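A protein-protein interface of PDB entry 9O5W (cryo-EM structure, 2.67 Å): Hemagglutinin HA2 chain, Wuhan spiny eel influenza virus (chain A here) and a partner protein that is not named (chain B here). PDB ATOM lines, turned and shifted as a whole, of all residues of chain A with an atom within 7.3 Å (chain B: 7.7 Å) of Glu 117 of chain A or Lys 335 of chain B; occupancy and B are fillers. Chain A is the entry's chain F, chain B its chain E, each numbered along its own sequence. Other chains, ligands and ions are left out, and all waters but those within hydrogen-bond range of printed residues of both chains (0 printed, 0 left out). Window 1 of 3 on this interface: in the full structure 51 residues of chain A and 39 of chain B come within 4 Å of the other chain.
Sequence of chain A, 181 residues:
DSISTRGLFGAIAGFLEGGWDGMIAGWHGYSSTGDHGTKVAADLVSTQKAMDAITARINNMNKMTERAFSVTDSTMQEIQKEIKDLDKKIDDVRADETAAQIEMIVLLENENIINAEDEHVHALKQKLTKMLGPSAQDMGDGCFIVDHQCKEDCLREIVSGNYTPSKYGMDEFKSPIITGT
Val 8 of chain B touches His 28 of chain A. CG1 of Val 331 of chain B touches CG2 of Ile 113 of chain A, 3.5 Å away. Lys 22 of chain B touches Ile 114 of chain A. CD1 of Ile 114 of chain A touches CG1 of Val 25 of chain B, 3.8 Å away. Ile 114 of chain A touches Lys 335 of chain B. Val 8 of chain B touches Glu 117 of chain A. Val 121 of chain A touches Gly 7 of chain B (CG2 to CA, 3.8 Å). Val 121 of chain A touches Val 8 of chain B (CG2 to CG1, 3.7 Å). Gly 7 of chain B touches Leu 124 of chain A.
Of the 19 printed residues of chain B, 6 touch a printed residue of chain A. Hydrophobic or aromatic side chains of chain B that line the printed part of chain A: Val 8, Val 25 and Val 331. Of the 16 printed residues of chain A, 8 touch a printed residue of chain B. Among the printed residues, 12 pairs touch across the chains.
Printed residues of chain B within 4 Å of Ile 114 of chain A: Lys 22 (3.7 Å), Val 25 (3.8 Å) and Lys 335 (3.7 Å). No residue of chain B comes within 4 Å of Ala 116 of chain A. Of the printed residues of chain B, Asp 118 of chain A touches Lys 335. Printed residues of chain A within 4 Å of Gly 7 of chain B: Val 121 and Leu 124. Of the printed residues of chain A, Val 8 of chain B touches His 28, Glu 117 and Val 121. Of the printed residues of chain A, Val 25 of chain B touches Ile 114 (3.8 Å). Leu 26 of chain B touches none of the printed residues of chain A. Of chain A, only Ile 114, Glu 117 and Asp 118 come within 4 Å of Lys 335 of chain B. The nearest residue of chain A that does not touch Lys 335 of chain B is Asn 115 of chain A (6.0 Å).
NZ of Lys 22 of chain B sits close to OD1 of Asn 115 of chain A (3.4 Å). The backbone NH of Lys 335 of chain B sits close to the side-chain carboxylate of Glu 117 of chain A, at 3.4 Å. The side-chain amino group (NZ) of Lys 335 of chain B lies within salt-bridge range of the side-chain carboxylate (OD2) of Asp 118 of chain A.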
ATOM      1  N   HIS A  28     -24.089 -18.415  11.871  1.00  0.00           N
ATOM      2  CA  HIS A  28     -24.246 -17.436  10.796  1.00  0.00           C
ATOM      3  C   HIS A  28     -24.134 -18.062   9.414  1.00  0.00           C
ATOM      4  O   HIS A  28     -23.344 -18.987   9.207  1.00  0.00           O
ATOM      5  CB  HIS A  28     -23.180 -16.343  10.926  1.00  0.00           C
ATOM      6  CG  HIS A  28     -23.322 -15.494  12.151  1.00  0.00           C
ATOM      7  ND1 HIS A  28     -24.029 -14.311  12.161  1.00  0.00           N
ATOM      8  CD2 HIS A  28     -22.851 -15.660  13.408  1.00  0.00           C
ATOM      9  CE1 HIS A  28     -23.981 -13.782  13.370  1.00  0.00           C
ATOM     10  NE2 HIS A  28     -23.274 -14.582  14.146  1.00  0.00           N
ATOM     11  N   ALA A  50     -17.981 -14.307  16.129  1.00  0.00           N
ATOM     12  CA  ALA A  50     -18.964 -14.072  17.182  1.00  0.00           C
ATOM     13  C   ALA A  50     -18.622 -14.869  18.430  1.00  0.00           C
ATOM     14  O   ALA A  50     -18.700 -14.357  19.556  1.00  0.00           O
ATOM     15  CB  ALA A  50     -20.360 -14.442  16.688  1.00  0.00           C
ATOM     16  N   GLU A 111     -26.536  -7.530  26.566  1.00  0.00           N
ATOM     17  CA  GLU A 111     -27.079  -6.595  25.585  1.00  0.00           C
ATOM     18  C   GLU A 111     -26.117  -6.424  24.413  1.00  0.00           C
ATOM     19  O   GLU A 111     -26.533  -6.414  23.247  1.00  0.00           O
ATOM     20  CB  GLU A 111     -27.353  -5.239  26.232  1.00  0.00           C
ATOM     21  CG  GLU A 111     -28.066  -4.260  25.304  1.00  0.00           C
ATOM     22  CD  GLU A 111     -28.378  -2.945  25.971  1.00  0.00           C
ATOM     23  OE1 GLU A 111     -29.172  -2.162  25.408  1.00  0.00           O
ATOM     24  OE2 GLU A 111     -27.774  -2.664  27.025  1.00  0.00           O
ATOM     25  N   ASN A 112     -24.817  -6.315  24.711  1.00  0.00           N
ATOM     26  CA  ASN A 112     -23.823  -6.126  23.659  1.00  0.00           C
ATOM     27  C   ASN A 112     -23.684  -7.362  22.781  1.00  0.00           C
ATOM     28  O   ASN A 112     -23.507  -7.241  21.563  1.00  0.00           O
ATOM     29  CB  ASN A 112     -22.479  -5.770  24.291  1.00  0.00           C
ATOM     30  CG  ASN A 112     -22.444  -4.352  24.830  1.00  0.00           C
ATOM     31  OD1 ASN A 112     -23.158  -3.473  24.350  1.00  0.00           O
ATOM     32  ND2 ASN A 112     -21.608  -4.124  25.833  1.00  0.00           N
ATOM     33  N   ILE A 113     -23.816  -8.551  23.366  1.00  0.00           N
ATOM     34  CA  ILE A 113     -23.731  -9.785  22.594  1.00  0.00           C
ATOM     35  C   ILE A 113     -24.915  -9.877  21.646  1.00  0.00           C
ATOM     36  O   ILE A 113     -24.764 -10.276  20.485  1.00  0.00           O
ATOM     37  CB  ILE A 113     -23.616 -11.011  23.525  1.00  0.00           C
ATOM     38  CG1 ILE A 113     -22.265 -10.990  24.253  1.00  0.00           C
ATOM     39  CG2 ILE A 113     -23.750 -12.336  22.738  1.00  0.00           C
ATOM     40  CD1 ILE A 113     -22.160 -11.937  25.443  1.00  0.00           C
ATOM     41  N   ILE A 114     -26.111  -9.530  22.122  1.00  0.00           N
ATOM     42  CA  ILE A 114     -27.273  -9.584  21.241  1.00  0.00           C
ATOM     43  C   ILE A 114     -27.135  -8.557  20.118  1.00  0.00           C
ATOM     44  O   ILE A 114     -27.438  -8.857  18.957  1.00  0.00           O
ATOM     45  CB  ILE A 114     -28.566  -9.398  22.064  1.00  0.00           C
ATOM     46  CG1 ILE A 114     -28.761 -10.599  23.002  1.00  0.00           C
ATOM     47  CG2 ILE A 114     -29.807  -9.251  21.153  1.00  0.00           C
ATOM     48  CD1 ILE A 114     -29.784 -10.395  24.101  1.00  0.00           C
ATOM     49  N   ASN A 115     -26.699  -7.331  20.433  1.00  0.00           N
ATOM     50  CA  ASN A 115     -26.535  -6.327  19.379  1.00  0.00           C
ATOM     51  C   ASN A 115     -25.480  -6.751  18.352  1.00  0.00           C
ATOM     52  O   ASN A 115     -25.580  -6.409  17.153  1.00  0.00           O
ATOM     53  CB  ASN A 115     -26.162  -4.984  20.008  1.00  0.00           C
ATOM     54  CG  ASN A 115     -27.340  -4.306  20.686  1.00  0.00           C
ATOM     55  OD1 ASN A 115     -28.499  -4.607  20.398  1.00  0.00           O
ATOM     56  ND2 ASN A 115     -27.049  -3.374  21.585  1.00  0.00           N
ATOM     57  N   ALA A 116     -24.448  -7.477  18.797  1.00  0.00           N
ATOM     58  CA  ALA A 116     -23.437  -7.931  17.853  1.00  0.00           C
ATOM     59  C   ALA A 116     -24.041  -8.827  16.779  1.00  0.00           C
ATOM     60  O   ALA A 116     -23.500  -8.905  15.672  1.00  0.00           O
ATOM     61  CB  ALA A 116     -22.322  -8.665  18.595  1.00  0.00           C
ATOM     62  N   GLU A 117     -25.152  -9.510  17.082  1.00  0.00           N
ATOM     63  CA  GLU A 117     -25.772 -10.387  16.093  1.00  0.00           C
ATOM     64  C   GLU A 117     -26.197  -9.577  14.876  1.00  0.00           C
ATOM     65  O   GLU A 117     -25.986  -9.990  13.726  1.00  0.00           O
ATOM     66  CB  GLU A 117     -26.962 -11.115  16.721  1.00  0.00           C
ATOM     67  CG  GLU A 117     -27.617 -12.180  15.851  1.00  0.00           C
ATOM     68  CD  GLU A 117     -29.119 -12.220  16.026  1.00  0.00           C
ATOM     69  OE1 GLU A 117     -29.589 -12.878  16.979  1.00  0.00           O
ATOM     70  OE2 GLU A 117     -29.832 -11.592  15.214  1.00  0.00           O
ATOM     71  N   ASP A 118     -26.667  -8.353  15.116  1.00  0.00           N
ATOM     72  CA  ASP A 118     -27.142  -7.526  14.025  1.00  0.00           C
ATOM     73  C   ASP A 118     -25.959  -6.888  13.334  1.00  0.00           C
ATOM     74  O   ASP A 118     -25.997  -6.667  12.117  1.00  0.00           O
ATOM     75  CB  ASP A 118     -28.102  -6.455  14.541  1.00  0.00           C
ATOM     76  CG  ASP A 118     -29.396  -7.039  15.067  1.00  0.00           C
ATOM     77  OD1 ASP A 118     -30.096  -7.727  14.295  1.00  0.00           O
ATOM     78  OD2 ASP A 118     -29.710  -6.812  16.255  1.00  0.00           O
ATOM     79  N   GLU A 119     -24.885  -6.627  14.085  1.00  0.00           N
ATOM     80  CA  GLU A 119     -23.697  -6.076  13.440  1.00  0.00           C
ATOM     81  C   GLU A 119     -23.114  -7.099  12.463  1.00  0.00           C
ATOM     82  O   GLU A 119     -22.707  -6.756  11.340  1.00  0.00           O
ATOM     83  CB  GLU A 119     -22.668  -5.674  14.494  1.00  0.00           C
ATOM     84  CG  GLU A 119     -23.071  -4.447  15.297  1.00  0.00           C
ATOM     85  CD  GLU A 119     -22.215  -4.244  16.530  1.00  0.00           C
ATOM     86  OE1 GLU A 119     -22.723  -3.670  17.518  1.00  0.00           O
ATOM     87  OE2 GLU A 119     -21.036  -4.656  16.515  1.00  0.00           O
ATOM     88  N   HIS A 120     -23.141  -8.377  12.854  1.00  0.00           N
ATOM     89  CA  HIS A 120     -22.609  -9.444  12.011  1.00  0.00           C
ATOM     90  C   HIS A 120     -23.491  -9.654  10.788  1.00  0.00           C
ATOM     91  O   HIS A 120     -22.987  -9.868   9.674  1.00  0.00           O
ATOM     92  CB  HIS A 120     -22.485 -10.747  12.805  1.00  0.00           C
ATOM     93  CG  HIS A 120     -21.417 -10.723  13.855  1.00  0.00           C
ATOM     94  ND1 HIS A 120     -20.093 -10.473  13.565  1.00  0.00           N
ATOM     95  CD2 HIS A 120     -21.468 -10.969  15.185  1.00  0.00           C
ATOM     96  CE1 HIS A 120     -19.382 -10.528  14.677  1.00  0.00           C
ATOM     97  NE2 HIS A 120     -20.193 -10.834  15.674  1.00  0.00           N
ATOM     98  N   VAL A 121     -24.813  -9.568  10.962  1.00  0.00           N
ATOM     99  CA  VAL A 121     -25.685  -9.725   9.803  1.00  0.00           C
ATOM    100  C   VAL A 121     -25.475  -8.564   8.843  1.00  0.00           C
ATOM    101  O   VAL A 121     -25.534  -8.743   7.621  1.00  0.00           O
ATOM    102  CB  VAL A 121     -27.159  -9.867  10.238  1.00  0.00           C
ATOM    103  CG1 VAL A 121     -28.112  -9.849   9.034  1.00  0.00           C
ATOM    104  CG2 VAL A 121     -27.354 -11.166  10.985  1.00  0.00           C
ATOM    105  N   HIS A 122     -25.296  -7.348   9.366  1.00  0.00           N
ATOM    106  CA  HIS A 122     -25.021  -6.217   8.485  1.00  0.00           C
ATOM    107  C   HIS A 122     -23.756  -6.463   7.668  1.00  0.00           C
ATOM    108  O   HIS A 122     -23.712  -6.159   6.466  1.00  0.00           O
ATOM    109  CB  HIS A 122     -24.891  -4.926   9.286  1.00  0.00           C
ATOM    110  CG  HIS A 122     -24.660  -3.720   8.431  1.00  0.00           C
ATOM    111  ND1 HIS A 122     -25.655  -3.147   7.669  1.00  0.00           N
ATOM    112  CD2 HIS A 122     -23.544  -2.988   8.203  1.00  0.00           C
ATOM    113  CE1 HIS A 122     -25.166  -2.109   7.016  1.00  0.00           C
ATOM    114  NE2 HIS A 122     -23.887  -1.991   7.321  1.00  0.00           N
ATOM    115  N   ALA A 123     -22.694  -6.958   8.318  1.00  0.00           N
ATOM    116  CA  ALA A 123     -21.468  -7.250   7.575  1.00  0.00           C
ATOM    117  C   ALA A 123     -21.722  -8.273   6.470  1.00  0.00           C
ATOM    118  O   ALA A 123     -21.203  -8.140   5.350  1.00  0.00           O
ATOM    119  CB  ALA A 123     -20.385  -7.753   8.528  1.00  0.00           C
ATOM    120  N   LEU A 124     -22.549  -9.286   6.754  1.00  0.00           N
ATOM    121  CA  LEU A 124     -22.850 -10.281   5.726  1.00  0.00           C
ATOM    122  C   LEU A 124     -23.626  -9.643   4.579  1.00  0.00           C
ATOM    123  O   LEU A 124     -23.414  -9.977   3.402  1.00  0.00           O
ATOM    124  CB  LEU A 124     -23.642 -11.442   6.327  1.00  0.00           C
ATOM    125  CG  LEU A 124     -22.954 -12.345   7.354  1.00  0.00           C
ATOM    126  CD1 LEU A 124     -23.960 -13.328   7.925  1.00  0.00           C
ATOM    127  CD2 LEU A 124     -21.772 -13.095   6.764  1.00  0.00           C
ATOM    128  N   GLY B   7     -28.254 -13.688   7.116  1.00  0.00           N
ATOM    129  CA  GLY B   7     -28.895 -13.575   8.409  1.00  0.00           C
ATOM    130  C   GLY B   7     -28.333 -14.601   9.359  1.00  0.00           C
ATOM    131  O   GLY B   7     -27.206 -15.071   9.193  1.00  0.00           O
ATOM    132  N   VAL B   8     -29.142 -14.947  10.360  1.00  0.00           N
ATOM    133  CA  VAL B   8     -28.788 -15.956  11.346  1.00  0.00           C
ATOM    134  C   VAL B   8     -29.911 -16.979  11.322  1.00  0.00           C
ATOM    135  O   VAL B   8     -31.038 -16.695  10.909  1.00  0.00           O
ATOM    136  CB  VAL B   8     -28.571 -15.384  12.768  1.00  0.00           C
ATOM    137  CG1 VAL B   8     -27.419 -14.399  12.770  1.00  0.00           C
ATOM    138  CG2 VAL B   8     -29.831 -14.701  13.305  1.00  0.00           C
ATOM    139  N   ALA B   9     -29.586 -18.179  11.780  1.00  0.00           N
ATOM    140  CA  ALA B   9     -30.537 -19.278  11.840  1.00  0.00           C
ATOM    141  C   ALA B   9     -31.251 -19.355  13.175  1.00  0.00           C
ATOM    142  O   ALA B   9     -30.710 -18.997  14.224  1.00  0.00           O
ATOM    143  CB  ALA B   9     -29.844 -20.601  11.569  1.00  0.00           C
ATOM    144  N   SER B  10     -32.480 -19.842  13.118  1.00  0.00           N
ATOM    145  CA  SER B  10     -33.280 -20.078  14.300  1.00  0.00           C
ATOM    146  C   SER B  10     -32.985 -21.447  14.899  1.00  0.00           C
ATOM    147  O   SER B  10     -32.298 -22.290  14.317  1.00  0.00           O
ATOM    148  CB  SER B  10     -34.764 -19.981  13.957  1.00  0.00           C
ATOM    149  OG  SER B  10     -35.144 -21.024  13.078  1.00  0.00           O
ATOM    150  N   GLY B  11     -33.521 -21.642  16.092  1.00  0.00           N
ATOM    151  CA  GLY B  11     -33.451 -22.894  16.817  1.00  0.00           C
ATOM    152  C   GLY B  11     -34.355 -22.739  18.013  1.00  0.00           C
ATOM    153  O   GLY B  11     -34.929 -21.671  18.242  1.00  0.00           O
ATOM    154  N   LYS B  12     -34.479 -23.803  18.793  1.00  0.00           N
ATOM    155  CA  LYS B  12     -35.352 -23.725  19.950  1.00  0.00           C
ATOM    156  C   LYS B  12     -34.627 -22.998  21.071  1.00  0.00           C
ATOM    157  O   LYS B  12     -33.414 -23.148  21.246  1.00  0.00           O
ATOM    158  CB  LYS B  12     -35.813 -25.133  20.359  1.00  0.00           C
ATOM    159  CG  LYS B  12     -34.770 -26.090  21.013  1.00  0.00           C
ATOM    160  CD  LYS B  12     -35.330 -26.932  22.171  1.00  0.00           C
ATOM    161  CE  LYS B  12     -35.728 -26.087  23.361  1.00  0.00           C
ATOM    162  NZ  LYS B  12     -35.932 -26.847  24.625  1.00  0.00           N
ATOM    163  N   GLY B  13     -35.370 -22.193  21.824  1.00  0.00           N
ATOM    164  CA  GLY B  13     -34.773 -21.514  22.953  1.00  0.00           C
ATOM    165  C   GLY B  13     -34.543 -22.482  24.092  1.00  0.00           C
ATOM    166  O   GLY B  13     -35.390 -23.322  24.397  1.00  0.00           O
ATOM    167  N   LYS B  22     -33.840  -5.074  26.744  1.00  0.00           N
ATOM    168  CA  LYS B  22     -34.587  -6.020  25.919  1.00  0.00           C
ATOM    169  C   LYS B  22     -35.421  -6.974  26.767  1.00  0.00           C
ATOM    170  O   LYS B  22     -36.102  -7.844  26.216  1.00  0.00           O
ATOM    171  CB  LYS B  22     -33.646  -6.809  24.986  1.00  0.00           C
ATOM    172  CG  LYS B  22     -32.889  -5.955  23.990  1.00  0.00           C
ATOM    173  CD  LYS B  22     -31.918  -6.797  23.173  1.00  0.00           C
ATOM    174  CE  LYS B  22     -31.040  -5.940  22.276  1.00  0.00           C
ATOM    175  NZ  LYS B  22     -31.786  -5.285  21.174  1.00  0.00           N
ATOM    176  N   VAL B  25     -34.487 -12.090  27.254  1.00  0.00           N
ATOM    177  CA  VAL B  25     -34.401 -12.507  25.862  1.00  0.00           C
ATOM    178  C   VAL B  25     -34.188 -14.011  25.820  1.00  0.00           C
ATOM    179  O   VAL B  25     -33.288 -14.534  26.485  1.00  0.00           O
ATOM    180  CB  VAL B  25     -33.264 -11.759  25.141  1.00  0.00           C
ATOM    181  CG1 VAL B  25     -33.110 -12.221  23.692  1.00  0.00           C
ATOM    182  CG2 VAL B  25     -33.496 -10.255  25.186  1.00  0.00           C
ATOM    183  N   LEU B  26     -35.013 -14.707  25.045  1.00  0.00           N
ATOM    184  CA  LEU B  26     -34.870 -16.148  24.902  1.00  0.00           C
ATOM    185  C   LEU B  26     -33.763 -16.438  23.898  1.00  0.00           C
ATOM    186  O   LEU B  26     -33.779 -15.917  22.778  1.00  0.00           O
ATOM    187  CB  LEU B  26     -36.191 -16.763  24.436  1.00  0.00           C
ATOM    188  CG  LEU B  26     -36.291 -18.283  24.262  1.00  0.00           C
ATOM    189  CD1 LEU B  26     -36.203 -19.033  25.571  1.00  0.00           C
ATOM    190  CD2 LEU B  26     -37.575 -18.646  23.535  1.00  0.00           C
ATOM    191  N   VAL B  27     -32.803 -17.270  24.303  1.00  0.00           N
ATOM    192  CA  VAL B  27     -31.656 -17.629  23.486  1.00  0.00           C
ATOM    193  C   VAL B  27     -31.557 -19.146  23.406  1.00  0.00           C
ATOM    194  O   VAL B  27     -32.035 -19.880  24.281  1.00  0.00           O
ATOM    195  CB  VAL B  27     -30.341 -17.013  24.025  1.00  0.00           C
ATOM    196  CG1 VAL B  27     -30.421 -15.496  24.003  1.00  0.00           C
ATOM    197  CG2 VAL B  27     -30.037 -17.489  25.447  1.00  0.00           C
ATOM    198  N   THR B  28     -30.840 -19.594  22.372  1.00  0.00           N
ATOM    199  CA  THR B  28     -30.654 -21.012  22.104  1.00  0.00           C
ATOM    200  C   THR B  28     -29.590 -21.650  22.981  1.00  0.00           C
ATOM    201  O   THR B  28     -29.590 -22.876  23.135  1.00  0.00           O
ATOM    202  CB  THR B  28     -30.275 -21.219  20.634  1.00  0.00           C
ATOM    203  OG1 THR B  28     -29.015 -20.587  20.373  1.00  0.00           O
ATOM    204  CG2 THR B  28     -31.336 -20.639  19.702  1.00  0.00           C
ATOM    205  N   ASN B  29     -28.683 -20.862  23.552  1.00  0.00           N
ATOM    206  CA  ASN B  29     -27.701 -21.408  24.474  1.00  0.00           C
ATOM    207  C   ASN B  29     -27.215 -20.294  25.384  1.00  0.00           C
ATOM    208  O   ASN B  29     -27.291 -19.111  25.044  1.00  0.00           O
ATOM    209  CB  ASN B  29     -26.524 -22.030  23.714  1.00  0.00           C
ATOM    210  CG  ASN B  29     -25.717 -22.995  24.558  1.00  0.00           C
ATOM    211  OD1 ASN B  29     -26.060 -23.283  25.704  1.00  0.00           O
ATOM    212  ND2 ASN B  29     -24.620 -23.485  23.995  1.00  0.00           N
ATOM    213  N   VAL B 331     -24.999 -14.927  27.170  1.00  0.00           N
ATOM    214  CA  VAL B 331     -25.420 -15.397  25.855  1.00  0.00           C
ATOM    215  C   VAL B 331     -24.258 -16.083  25.155  1.00  0.00           C
ATOM    216  O   VAL B 331     -23.148 -15.541  25.083  1.00  0.00           O
ATOM    217  CB  VAL B 331     -25.937 -14.220  25.008  1.00  0.00           C
ATOM    218  CG1 VAL B 331     -26.286 -14.645  23.568  1.00  0.00           C
ATOM    219  CG2 VAL B 331     -27.126 -13.603  25.641  1.00  0.00           C
ATOM    220  N   GLY B 333     -24.997 -17.908  21.954  1.00  0.00           N
ATOM    221  CA  GLY B 333     -25.806 -18.414  20.860  1.00  0.00           C
ATOM    222  C   GLY B 333     -26.619 -17.279  20.287  1.00  0.00           C
ATOM    223  O   GLY B 333     -26.500 -16.126  20.712  1.00  0.00           O
ATOM    224  N   THR B 334     -27.456 -17.615  19.312  1.00  0.00           N
ATOM    225  CA  THR B 334     -28.288 -16.600  18.688  1.00  0.00           C
ATOM    226  C   THR B 334     -29.568 -16.408  19.495  1.00  0.00           C
ATOM    227  O   THR B 334     -29.934 -17.224  20.342  1.00  0.00           O
ATOM    228  CB  THR B 334     -28.641 -16.986  17.250  1.00  0.00           C
ATOM    229  OG1 THR B 334     -29.372 -18.219  17.247  1.00  0.00           O
ATOM    230  CG2 THR B 334     -27.389 -17.136  16.399  1.00  0.00           C
ATOM    231  N   LYS B 335     -30.250 -15.301  19.224  1.00  0.00           N
ATOM    232  CA  LYS B 335     -31.546 -15.054  19.834  1.00  0.00           C
ATOM    233  C   LYS B 335     -32.564 -16.056  19.295  1.00  0.00           C
ATOM    234  O   LYS B 335     -32.605 -16.339  18.095  1.00  0.00           O
ATOM    235  CB  LYS B 335     -31.954 -13.602  19.590  1.00  0.00           C
ATOM    236  CG  LYS B 335     -32.127 -13.214  18.136  1.00  0.00           C
ATOM    237  CD  LYS B 335     -32.542 -11.737  17.885  1.00  0.00           C
ATOM    238  CE  LYS B 335     -31.555 -10.580  18.200  1.00  0.00           C
ATOM    239  NZ  LYS B 335     -31.907  -9.145  17.976  1.00  0.00           N
ATOM    240  N   ALA B 336     -33.388 -16.597  20.188  1.00  0.00           N
ATOM    241  CA  ALA B 336     -34.382 -17.587  19.799  1.00  0.00           C
ATOM    242  C   ALA B 336     -35.514 -16.979  18.979  1.00  0.00           C
ATOM    243  O   ALA B 336     -35.914 -15.830  19.174  1.00  0.00           O
ATOM    244  CB  ALA B 336     -34.962 -18.275  21.031  1.00  0.00           C
ATOM    245  N   ARG B 337     -36.030 -17.784  18.053  1.00  0.00           N
ATOM    246  CA  ARG B 337     -37.165 -17.416  17.214  1.00  0.00           C
ATOM    247  C   ARG B 337     -38.452 -17.404  18.032  1.00  0.00           C
ATOM    248  O   ARG B 337     -39.395 -16.680  17.713  1.00  0.00           O
ATOM    249  CB  ARG B 337     -37.279 -18.405  16.051  1.00  0.00           C
ATOM    250  CG  ARG B 337     -38.368 -18.139  15.016  1.00  0.00           C
ATOM    251  CD  ARG B 337     -38.128 -16.870  14.224  1.00  0.00           C
ATOM    252  NE  ARG B 337     -39.055 -16.764  13.103  1.00  0.00           N
ATOM    253  CZ  ARG B 337     -39.194 -15.696  12.327  1.00  0.00           C
ATOM    254  NH1 ARG B 337     -38.477 -14.598  12.517  1.00  0.00           N
ATOM    255  NH2 ARG B 337     -40.074 -15.730  11.331  1.00  0.00           N
